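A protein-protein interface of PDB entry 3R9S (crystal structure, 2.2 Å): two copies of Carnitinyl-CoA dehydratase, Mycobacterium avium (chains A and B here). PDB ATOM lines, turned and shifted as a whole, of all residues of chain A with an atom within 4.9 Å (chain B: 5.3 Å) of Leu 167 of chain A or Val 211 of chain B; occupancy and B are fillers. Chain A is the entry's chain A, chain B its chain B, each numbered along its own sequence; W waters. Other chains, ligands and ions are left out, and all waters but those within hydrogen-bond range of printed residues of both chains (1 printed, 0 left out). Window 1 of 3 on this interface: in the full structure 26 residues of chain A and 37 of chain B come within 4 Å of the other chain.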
ATOM      1  N   VAL A 139      31.691  19.425   5.518  1.00  0.00           N
ATOM      2  CA  VAL A 139      31.958  18.203   6.272  1.00  0.00           C
ATOM      3  C   VAL A 139      33.000  17.297   5.623  1.00  0.00           C
ATOM      4  O   VAL A 139      33.604  16.480   6.307  1.00  0.00           O
ATOM      5  CB  VAL A 139      30.668  17.373   6.579  1.00  0.00           C
ATOM      6  CG1 VAL A 139      29.721  18.137   7.549  1.00  0.00           C
ATOM      7  CG2 VAL A 139      29.959  16.941   5.311  1.00  0.00           C
ATOM      8  N   MET A 163      18.831  17.278   5.404  1.00  0.00           N
ATOM      9  CA  MET A 163      19.792  16.461   6.174  1.00  0.00           C
ATOM     10  C   MET A 163      20.777  15.686   5.292  1.00  0.00           C
ATOM     11  O   MET A 163      21.966  15.580   5.636  1.00  0.00           O
ATOM     12  CB  MET A 163      19.073  15.481   7.105  1.00  0.00           C
ATOM     13  CG  MET A 163      18.248  16.117   8.213  1.00  0.00           C
ATOM     14  SD  MET A 163      19.073  17.424   9.152  1.00  0.00           S
ATOM     15  CE  MET A 163      20.455  16.469   9.788  1.00  0.00           C
ATOM     16  N   ARG A 164      20.287  15.117   4.189  1.00  0.00           N
ATOM     17  CA  ARG A 164      21.142  14.425   3.216  1.00  0.00           C
ATOM     18  C   ARG A 164      22.264  15.357   2.735  1.00  0.00           C
ATOM     19  O   ARG A 164      23.443  14.995   2.721  1.00  0.00           O
ATOM     20  CB  ARG A 164      20.298  13.975   2.023  1.00  0.00           C
ATOM     21  CG  ARG A 164      21.060  13.283   0.894  1.00  0.00           C
ATOM     22  CD  ARG A 164      20.093  12.819  -0.208  1.00  0.00           C
ATOM     23  NE  ARG A 164      20.495  11.546  -0.791  1.00  0.00           N
ATOM     24  CZ  ARG A 164      19.727  10.777  -1.569  1.00  0.00           C
ATOM     25  NH1 ARG A 164      20.216   9.633  -2.007  1.00  0.00           N
ATOM     26  NH2 ARG A 164      18.485  11.134  -1.911  1.00  0.00           N
ATOM     27  N   LEU A 165      21.861  16.558   2.324  1.00  0.00           N
ATOM     28  CA  LEU A 165      22.788  17.551   1.793  1.00  0.00           C
ATOM     29  C   LEU A 165      23.845  17.894   2.847  1.00  0.00           C
ATOM     30  O   LEU A 165      25.057  17.892   2.582  1.00  0.00           O
ATOM     31  CB  LEU A 165      21.989  18.782   1.363  1.00  0.00           C
ATOM     32  CG  LEU A 165      22.635  19.898   0.554  1.00  0.00           C
ATOM     33  CD1 LEU A 165      21.546  20.658  -0.221  1.00  0.00           C
ATOM     34  CD2 LEU A 165      23.401  20.822   1.461  1.00  0.00           C
ATOM     35  N   LEU A 166      23.369  18.158   4.058  1.00  0.00           N
ATOM     36  CA  LEU A 166      24.225  18.587   5.159  1.00  0.00           C
ATOM     37  C   LEU A 166      25.204  17.499   5.591  1.00  0.00           C
ATOM     38  O   LEU A 166      26.383  17.786   5.865  1.00  0.00           O
ATOM     39  CB  LEU A 166      23.348  18.977   6.347  1.00  0.00           C
ATOM     40  CG  LEU A 166      24.004  19.600   7.562  1.00  0.00           C
ATOM     41  CD1 LEU A 166      24.623  20.983   7.234  1.00  0.00           C
ATOM     42  CD2 LEU A 166      22.963  19.704   8.648  1.00  0.00           C
ATOM     43  N   LEU A 167      24.723  16.263   5.655  1.00  0.00           N
ATOM     44  CA  LEU A 167      25.523  15.163   6.205  1.00  0.00           C
ATOM     45  C   LEU A 167      26.390  14.462   5.154  1.00  0.00           C
ATOM     46  O   LEU A 167      27.450  13.944   5.505  1.00  0.00           O
ATOM     47  CB  LEU A 167      24.646  14.122   6.915  1.00  0.00           C
ATOM     48  CG  LEU A 167      23.713  14.651   8.011  1.00  0.00           C
ATOM     49  CD1 LEU A 167      22.842  13.559   8.625  1.00  0.00           C
ATOM     50  CD2 LEU A 167      24.472  15.396   9.058  1.00  0.00           C
ATOM     51  N   THR A 168      25.970  14.445   3.886  1.00  0.00           N
ATOM     52  CA  THR A 168      26.800  13.843   2.820  1.00  0.00           C
ATOM     53  C   THR A 168      27.801  14.851   2.205  1.00  0.00           C
ATOM     54  O   THR A 168      28.825  14.451   1.656  1.00  0.00           O
ATOM     55  CB  THR A 168      25.962  13.228   1.669  1.00  0.00           C
ATOM     56  OG1 THR A 168      25.358  14.265   0.886  1.00  0.00           O
ATOM     57  CG2 THR A 168      24.880  12.310   2.218  1.00  0.00           C
ATOM     58  N   GLY A 169      27.493  16.147   2.286  1.00  0.00           N
ATOM     59  CA  GLY A 169      28.293  17.178   1.619  1.00  0.00           C
ATOM     60  C   GLY A 169      28.274  17.165   0.092  1.00  0.00           C
ATOM     61  O   GLY A 169      29.097  17.822  -0.555  1.00  0.00           O
ATOM     62  N   PRO B 103      24.405   9.830  12.613  1.00  0.00           N
ATOM     63  CA  PRO B 103      23.259   9.864  11.715  1.00  0.00           C
ATOM     64  C   PRO B 103      22.560   8.512  11.558  1.00  0.00           C
ATOM     65  O   PRO B 103      23.227   7.457  11.512  1.00  0.00           O
ATOM     66  CB  PRO B 103      23.846  10.328  10.383  1.00  0.00           C
ATOM     67  CG  PRO B 103      25.134  11.008  10.715  1.00  0.00           C
ATOM     68  CD  PRO B 103      25.639  10.337  11.977  1.00  0.00           C
ATOM     69  N   ASP B 124      17.111  10.332  10.642  1.00  0.00           N
ATOM     70  CA  ASP B 124      17.611  11.470   9.869  1.00  0.00           C
ATOM     71  C   ASP B 124      17.298  11.373   8.398  1.00  0.00           C
ATOM     72  O   ASP B 124      16.960  12.377   7.748  1.00  0.00           O
ATOM     73  CB  ASP B 124      19.125  11.603  10.063  1.00  0.00           C
ATOM     74  CG  ASP B 124      19.485  11.824  11.510  1.00  0.00           C
ATOM     75  OD1 ASP B 124      18.783  12.661  12.144  1.00  0.00           O
ATOM     76  OD2 ASP B 124      20.410  11.147  12.014  1.00  0.00           O
ATOM     77  N   LEU B 125      17.403  10.150   7.888  1.00  0.00           N
ATOM     78  CA  LEU B 125      17.268   9.869   6.480  1.00  0.00           C
ATOM     79  C   LEU B 125      16.420   8.600   6.299  1.00  0.00           C
ATOM     80  O   LEU B 125      16.346   7.743   7.200  1.00  0.00           O
ATOM     81  CB  LEU B 125      18.658   9.669   5.890  1.00  0.00           C
ATOM     82  CG  LEU B 125      19.637  10.864   5.934  1.00  0.00           C
ATOM     83  CD1 LEU B 125      21.025  10.409   5.609  1.00  0.00           C
ATOM     84  CD2 LEU B 125      19.235  11.979   4.958  1.00  0.00           C
ATOM     85  N   ALA B 202      28.177   7.412   2.002  1.00  0.00           N
ATOM     86  CA  ALA B 202      28.345   8.793   1.563  1.00  0.00           C
ATOM     87  C   ALA B 202      28.463   9.771   2.755  1.00  0.00           C
ATOM     88  O   ALA B 202      28.913  10.908   2.573  1.00  0.00           O
ATOM     89  CB  ALA B 202      27.216   9.215   0.624  1.00  0.00           C
ATOM     90  N   ILE B 203      28.067   9.326   3.948  1.00  0.00           N
ATOM     91  CA  ILE B 203      28.162  10.114   5.181  1.00  0.00           C
ATOM     92  C   ILE B 203      29.400   9.727   6.006  1.00  0.00           C
ATOM     93  O   ILE B 203      30.117  10.599   6.517  1.00  0.00           O
ATOM     94  CB  ILE B 203      26.924   9.924   6.083  1.00  0.00           C
ATOM     95  CG1 ILE B 203      25.642  10.378   5.364  1.00  0.00           C
ATOM     96  CG2 ILE B 203      27.100  10.686   7.390  1.00  0.00           C
ATOM     97  CD1 ILE B 203      24.332   9.884   6.044  1.00  0.00           C
ATOM     98  N   ASN B 206      32.936  11.217   5.433  1.00  0.00           N
ATOM     99  CA  ASN B 206      33.196  12.563   5.931  1.00  0.00           C
ATOM    100  C   ASN B 206      33.738  12.619   7.354  1.00  0.00           C
ATOM    101  O   ASN B 206      33.694  11.616   8.101  1.00  0.00           O
ATOM    102  CB  ASN B 206      31.921  13.392   5.810  1.00  0.00           C
ATOM    103  CG  ASN B 206      31.413  13.445   4.380  1.00  0.00           C
ATOM    104  OD1 ASN B 206      32.207  13.454   3.443  1.00  0.00           O
ATOM    105  ND2 ASN B 206      30.098  13.450   4.207  1.00  0.00           N
ATOM    106  N   ALA B 207      34.271  13.788   7.723  1.00  0.00           N
ATOM    107  CA  ALA B 207      34.802  13.996   9.073  1.00  0.00           C
ATOM    108  C   ALA B 207      33.676  13.796  10.104  1.00  0.00           C
ATOM    109  O   ALA B 207      32.726  14.565  10.136  1.00  0.00           O
ATOM    110  CB  ALA B 207      35.408  15.380   9.201  1.00  0.00           C
ATOM    111  N   PRO B 208      33.768  12.745  10.927  1.00  0.00           N
ATOM    112  CA  PRO B 208      32.648  12.393  11.804  1.00  0.00           C
ATOM    113  C   PRO B 208      32.260  13.459  12.840  1.00  0.00           C
ATOM    114  O   PRO B 208      31.063  13.614  13.110  1.00  0.00           O
ATOM    115  CB  PRO B 208      33.106  11.094  12.481  1.00  0.00           C
ATOM    116  CG  PRO B 208      34.584  11.027  12.274  1.00  0.00           C
ATOM    117  CD  PRO B 208      34.875  11.776  11.020  1.00  0.00           C
ATOM    118  N   LEU B 209      33.229  14.205  13.387  1.00  0.00           N
ATOM    119  CA  LEU B 209      32.892  15.230  14.380  1.00  0.00           C
ATOM    120  C   LEU B 209      32.120  16.408  13.745  1.00  0.00           C
ATOM    121  O   LEU B 209      31.253  16.999  14.377  1.00  0.00           O
ATOM    122  CB  LEU B 209      34.136  15.752  15.119  1.00  0.00           C
ATOM    123  CG  LEU B 209      34.921  14.779  16.006  1.00  0.00           C
ATOM    124  CD1 LEU B 209      36.089  15.537  16.693  1.00  0.00           C
ATOM    125  CD2 LEU B 209      34.037  14.089  17.041  1.00  0.00           C
ATOM    126  N   SER B 210      32.446  16.730  12.496  1.00  0.00           N
ATOM    127  CA  SER B 210      31.761  17.779  11.757  1.00  0.00           C
ATOM    128  C   SER B 210      30.335  17.338  11.382  1.00  0.00           C
ATOM    129  O   SER B 210      29.391  18.118  11.486  1.00  0.00           O
ATOM    130  CB  SER B 210      32.550  18.121  10.498  1.00  0.00           C
ATOM    131  OG  SER B 210      33.885  18.483  10.811  1.00  0.00           O
ATOM    132  N   VAL B 211      30.195  16.091  10.944  1.00  0.00           N
ATOM    133  CA  VAL B 211      28.902  15.543  10.589  1.00  0.00           C
ATOM    134  C   VAL B 211      27.996  15.566  11.807  1.00  0.00           C
ATOM    135  O   VAL B 211      26.840  15.998  11.731  1.00  0.00           O
ATOM    136  CB  VAL B 211      29.028  14.076  10.076  1.00  0.00           C
ATOM    137  CG1 VAL B 211      27.679  13.370  10.074  1.00  0.00           C
ATOM    138  CG2 VAL B 211      29.638  14.047   8.695  1.00  0.00           C
ATOM    139  N   GLN B 212      28.554  15.111  12.931  1.00  0.00           N
ATOM    140  CA  GLN B 212      27.832  14.976  14.180  1.00  0.00           C
ATOM    141  C   GLN B 212      27.464  16.333  14.802  1.00  0.00           C
ATOM    142  O   GLN B 212      26.327  16.531  15.264  1.00  0.00           O
ATOM    143  CB  GLN B 212      28.624  14.063  15.127  1.00  0.00           C
ATOM    144  CG  GLN B 212      28.785  12.649  14.533  1.00  0.00           C
ATOM    145  CD  GLN B 212      29.788  11.753  15.253  1.00  0.00           C
ATOM    146  OE1 GLN B 212      30.291  10.783  14.679  1.00  0.00           O
ATOM    147  NE2 GLN B 212      30.057  12.050  16.507  1.00  0.00           N
ATOM    148  N   ALA B 213      28.393  17.274  14.781  1.00  0.00           N
ATOM    149  CA  ALA B 213      28.069  18.651  15.177  1.00  0.00           C
ATOM    150  C   ALA B 213      26.981  19.250  14.277  1.00  0.00           C
ATOM    151  O   ALA B 213      26.114  20.005  14.741  1.00  0.00           O
ATOM    152  CB  ALA B 213      29.323  19.528  15.135  1.00  0.00           C
ATOM    153  N   SER B 214      27.022  18.925  12.985  1.00  0.00           N
ATOM    154  CA  SER B 214      26.031  19.480  12.050  1.00  0.00           C
ATOM    155  C   SER B 214      24.637  18.939  12.389  1.00  0.00           C
ATOM    156  O   SER B 214      23.661  19.679  12.383  1.00  0.00           O
ATOM    157  CB  SER B 214      26.410  19.194  10.593  1.00  0.00           C
ATOM    158  OG  SER B 214      27.655  19.784  10.252  1.00  0.00           O
ATOM    159  N   LYS B 215      24.568  17.658  12.727  1.00  0.00           N
ATOM    160  CA  LYS B 215      23.324  17.037  13.132  1.00  0.00           C
ATOM    161  C   LYS B 215      22.746  17.717  14.379  1.00  0.00           C
ATOM    162  O   LYS B 215      21.568  18.096  14.386  1.00  0.00           O
ATOM    163  CB  LYS B 215      23.510  15.536  13.382  1.00  0.00           C
ATOM    164  CG  LYS B 215      22.205  14.828  13.700  1.00  0.00           C
ATOM    165  CD  LYS B 215      22.393  13.355  13.948  1.00  0.00           C
ATOM    166  CE  LYS B 215      21.174  12.738  14.639  1.00  0.00           C
ATOM    167  NZ  LYS B 215      21.243  11.259  14.549  1.00  0.00           N
ATOM    168  N   ARG B 216      23.569  17.885  15.410  1.00  0.00           N
ATOM    169  CA  ARG B 216      23.121  18.534  16.649  1.00  0.00           C
ATOM    170  C   ARG B 216      22.577  19.943  16.395  1.00  0.00           C
ATOM    171  O   ARG B 216      21.531  20.307  16.920  1.00  0.00           O
ATOM    172  CB  ARG B 216      24.260  18.597  17.687  1.00  0.00           C
ATOM    173  CG  ARG B 216      24.668  17.241  18.288  1.00  0.00           C
ATOM    174  CD  ARG B 216      25.576  17.415  19.502  1.00  0.00           C
ATOM    175  NE  ARG B 216      26.905  17.949  19.165  1.00  0.00           N
ATOM    176  CZ  ARG B 216      27.933  17.227  18.748  1.00  0.00           C
ATOM    177  NH1 ARG B 216      29.095  17.819  18.479  1.00  0.00           N
ATOM    178  NH2 ARG B 216      27.820  15.907  18.605  1.00  0.00           N
HETATM  179  O   HOH W   1      29.736  11.508   0.102  1.00  0.00           O
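The side-chain amide nitrogen of Asn 206 of chain B is in hydrogen-bond range of the backbone carbonyl oxygen of Leu 167 of chain A (3.0 Å). The side-chain amide nitrogen (ND2) of Asn 206 of chain B sits at hydrogen-bond distance from the backbone carbonyl oxygen (O) of Thr 168 of chain A, 3.0 Å away. The backbone carbonyl oxygen (O) of Val 139 of chain A lies within hydrogen-bond range of the backbone NH (N) of Ala 207 of chain B (3.1 Å).
The backbone carbonyl oxygen (O) of Ala 202 of chain B lies within hydrogen-bond range of the side-chain amide nitrogen (ND2) of Asn 206 of chain B (3.2 Å). The side-chain carboxylate (OD2) of Asp 124 of chain B lies within salt-bridge range of the side-chain amino group (NZ) of Lys 215 of chain B, at 2.7 Å. The backbone carbonyl oxygen (O) of Arg 164 of chain A lies within hydrogen-bond range of the side-chain hydroxyl (OG1) of Thr 168 of chain A (2.8 Å). The backbone carbonyl oxygen of Ser 210 of chain B sits at hydrogen-bond distance from the side-chain hydroxyl of Ser 214 of chain B (2.7 Å).
Asn 206 of chain B touches Val 139 of chain A. Val 139 of chain A touches Ser 210 of chain B (CG1 to O, 3.95 Å). Ser 214 of chain B touches Val 139 of chain A (OG to CG1, 3.8 Å). O of Asp 124 of chain B touches CB of Met 163 of chain A (3.8 Å). Leu 125 of chain B touches Arg 164 of chain A. Leu 166 of chain A touches Ser 214 of chain B (CD2 to O, 3.8 Å). Leu 167 of chain A touches Ile 203 of chain B. CD2 of Leu 167 of chain A touches O of Val 211 of chain B (3.6 Å). Thr 168 of chain A touches Ala 202 of chain B (CA to O, 3.6 Å). Ile 203 of chain B touches Thr 168 of chain A (CG1 to CG2, 3.8 Å).
Of chain B, only Pro 103, Ile 203, Asn 206 and Val 211 come within 4 Å of Leu 167 of chain A. Of the printed residues of chain A, Val 211 of chain B touches Val 139 and Leu 167. Of the printed residues of chain A, Ser 214 of chain B touches Val 139 (3.8 Å) and Leu 166 (3.8 Å). Of the printed residues of chain A, Pro 103 of chain B touches Leu 167. Of the printed residues of chain A, Ala 202 of chain B touches Thr 168 (3.6 Å). Gln 212 of chain B touches none of the printed residues of chain A. The nearest printed residue of chain B that does not touch Thr 168 of chain A is Leu 125 of chain B (5.5 Å).
Along chain B the printed residues that touch a printed residue of chain A span positions 103 to 214. Among the printed residues, 15 pairs touch across the chains.
No position is printed for both chains.
Water W1 bridges the backbone carbonyl oxygen of Ala 202 of chain B (2.7 Å) and the backbone carbonyl oxygen of Thr 168 of chain A (3.5 Å).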
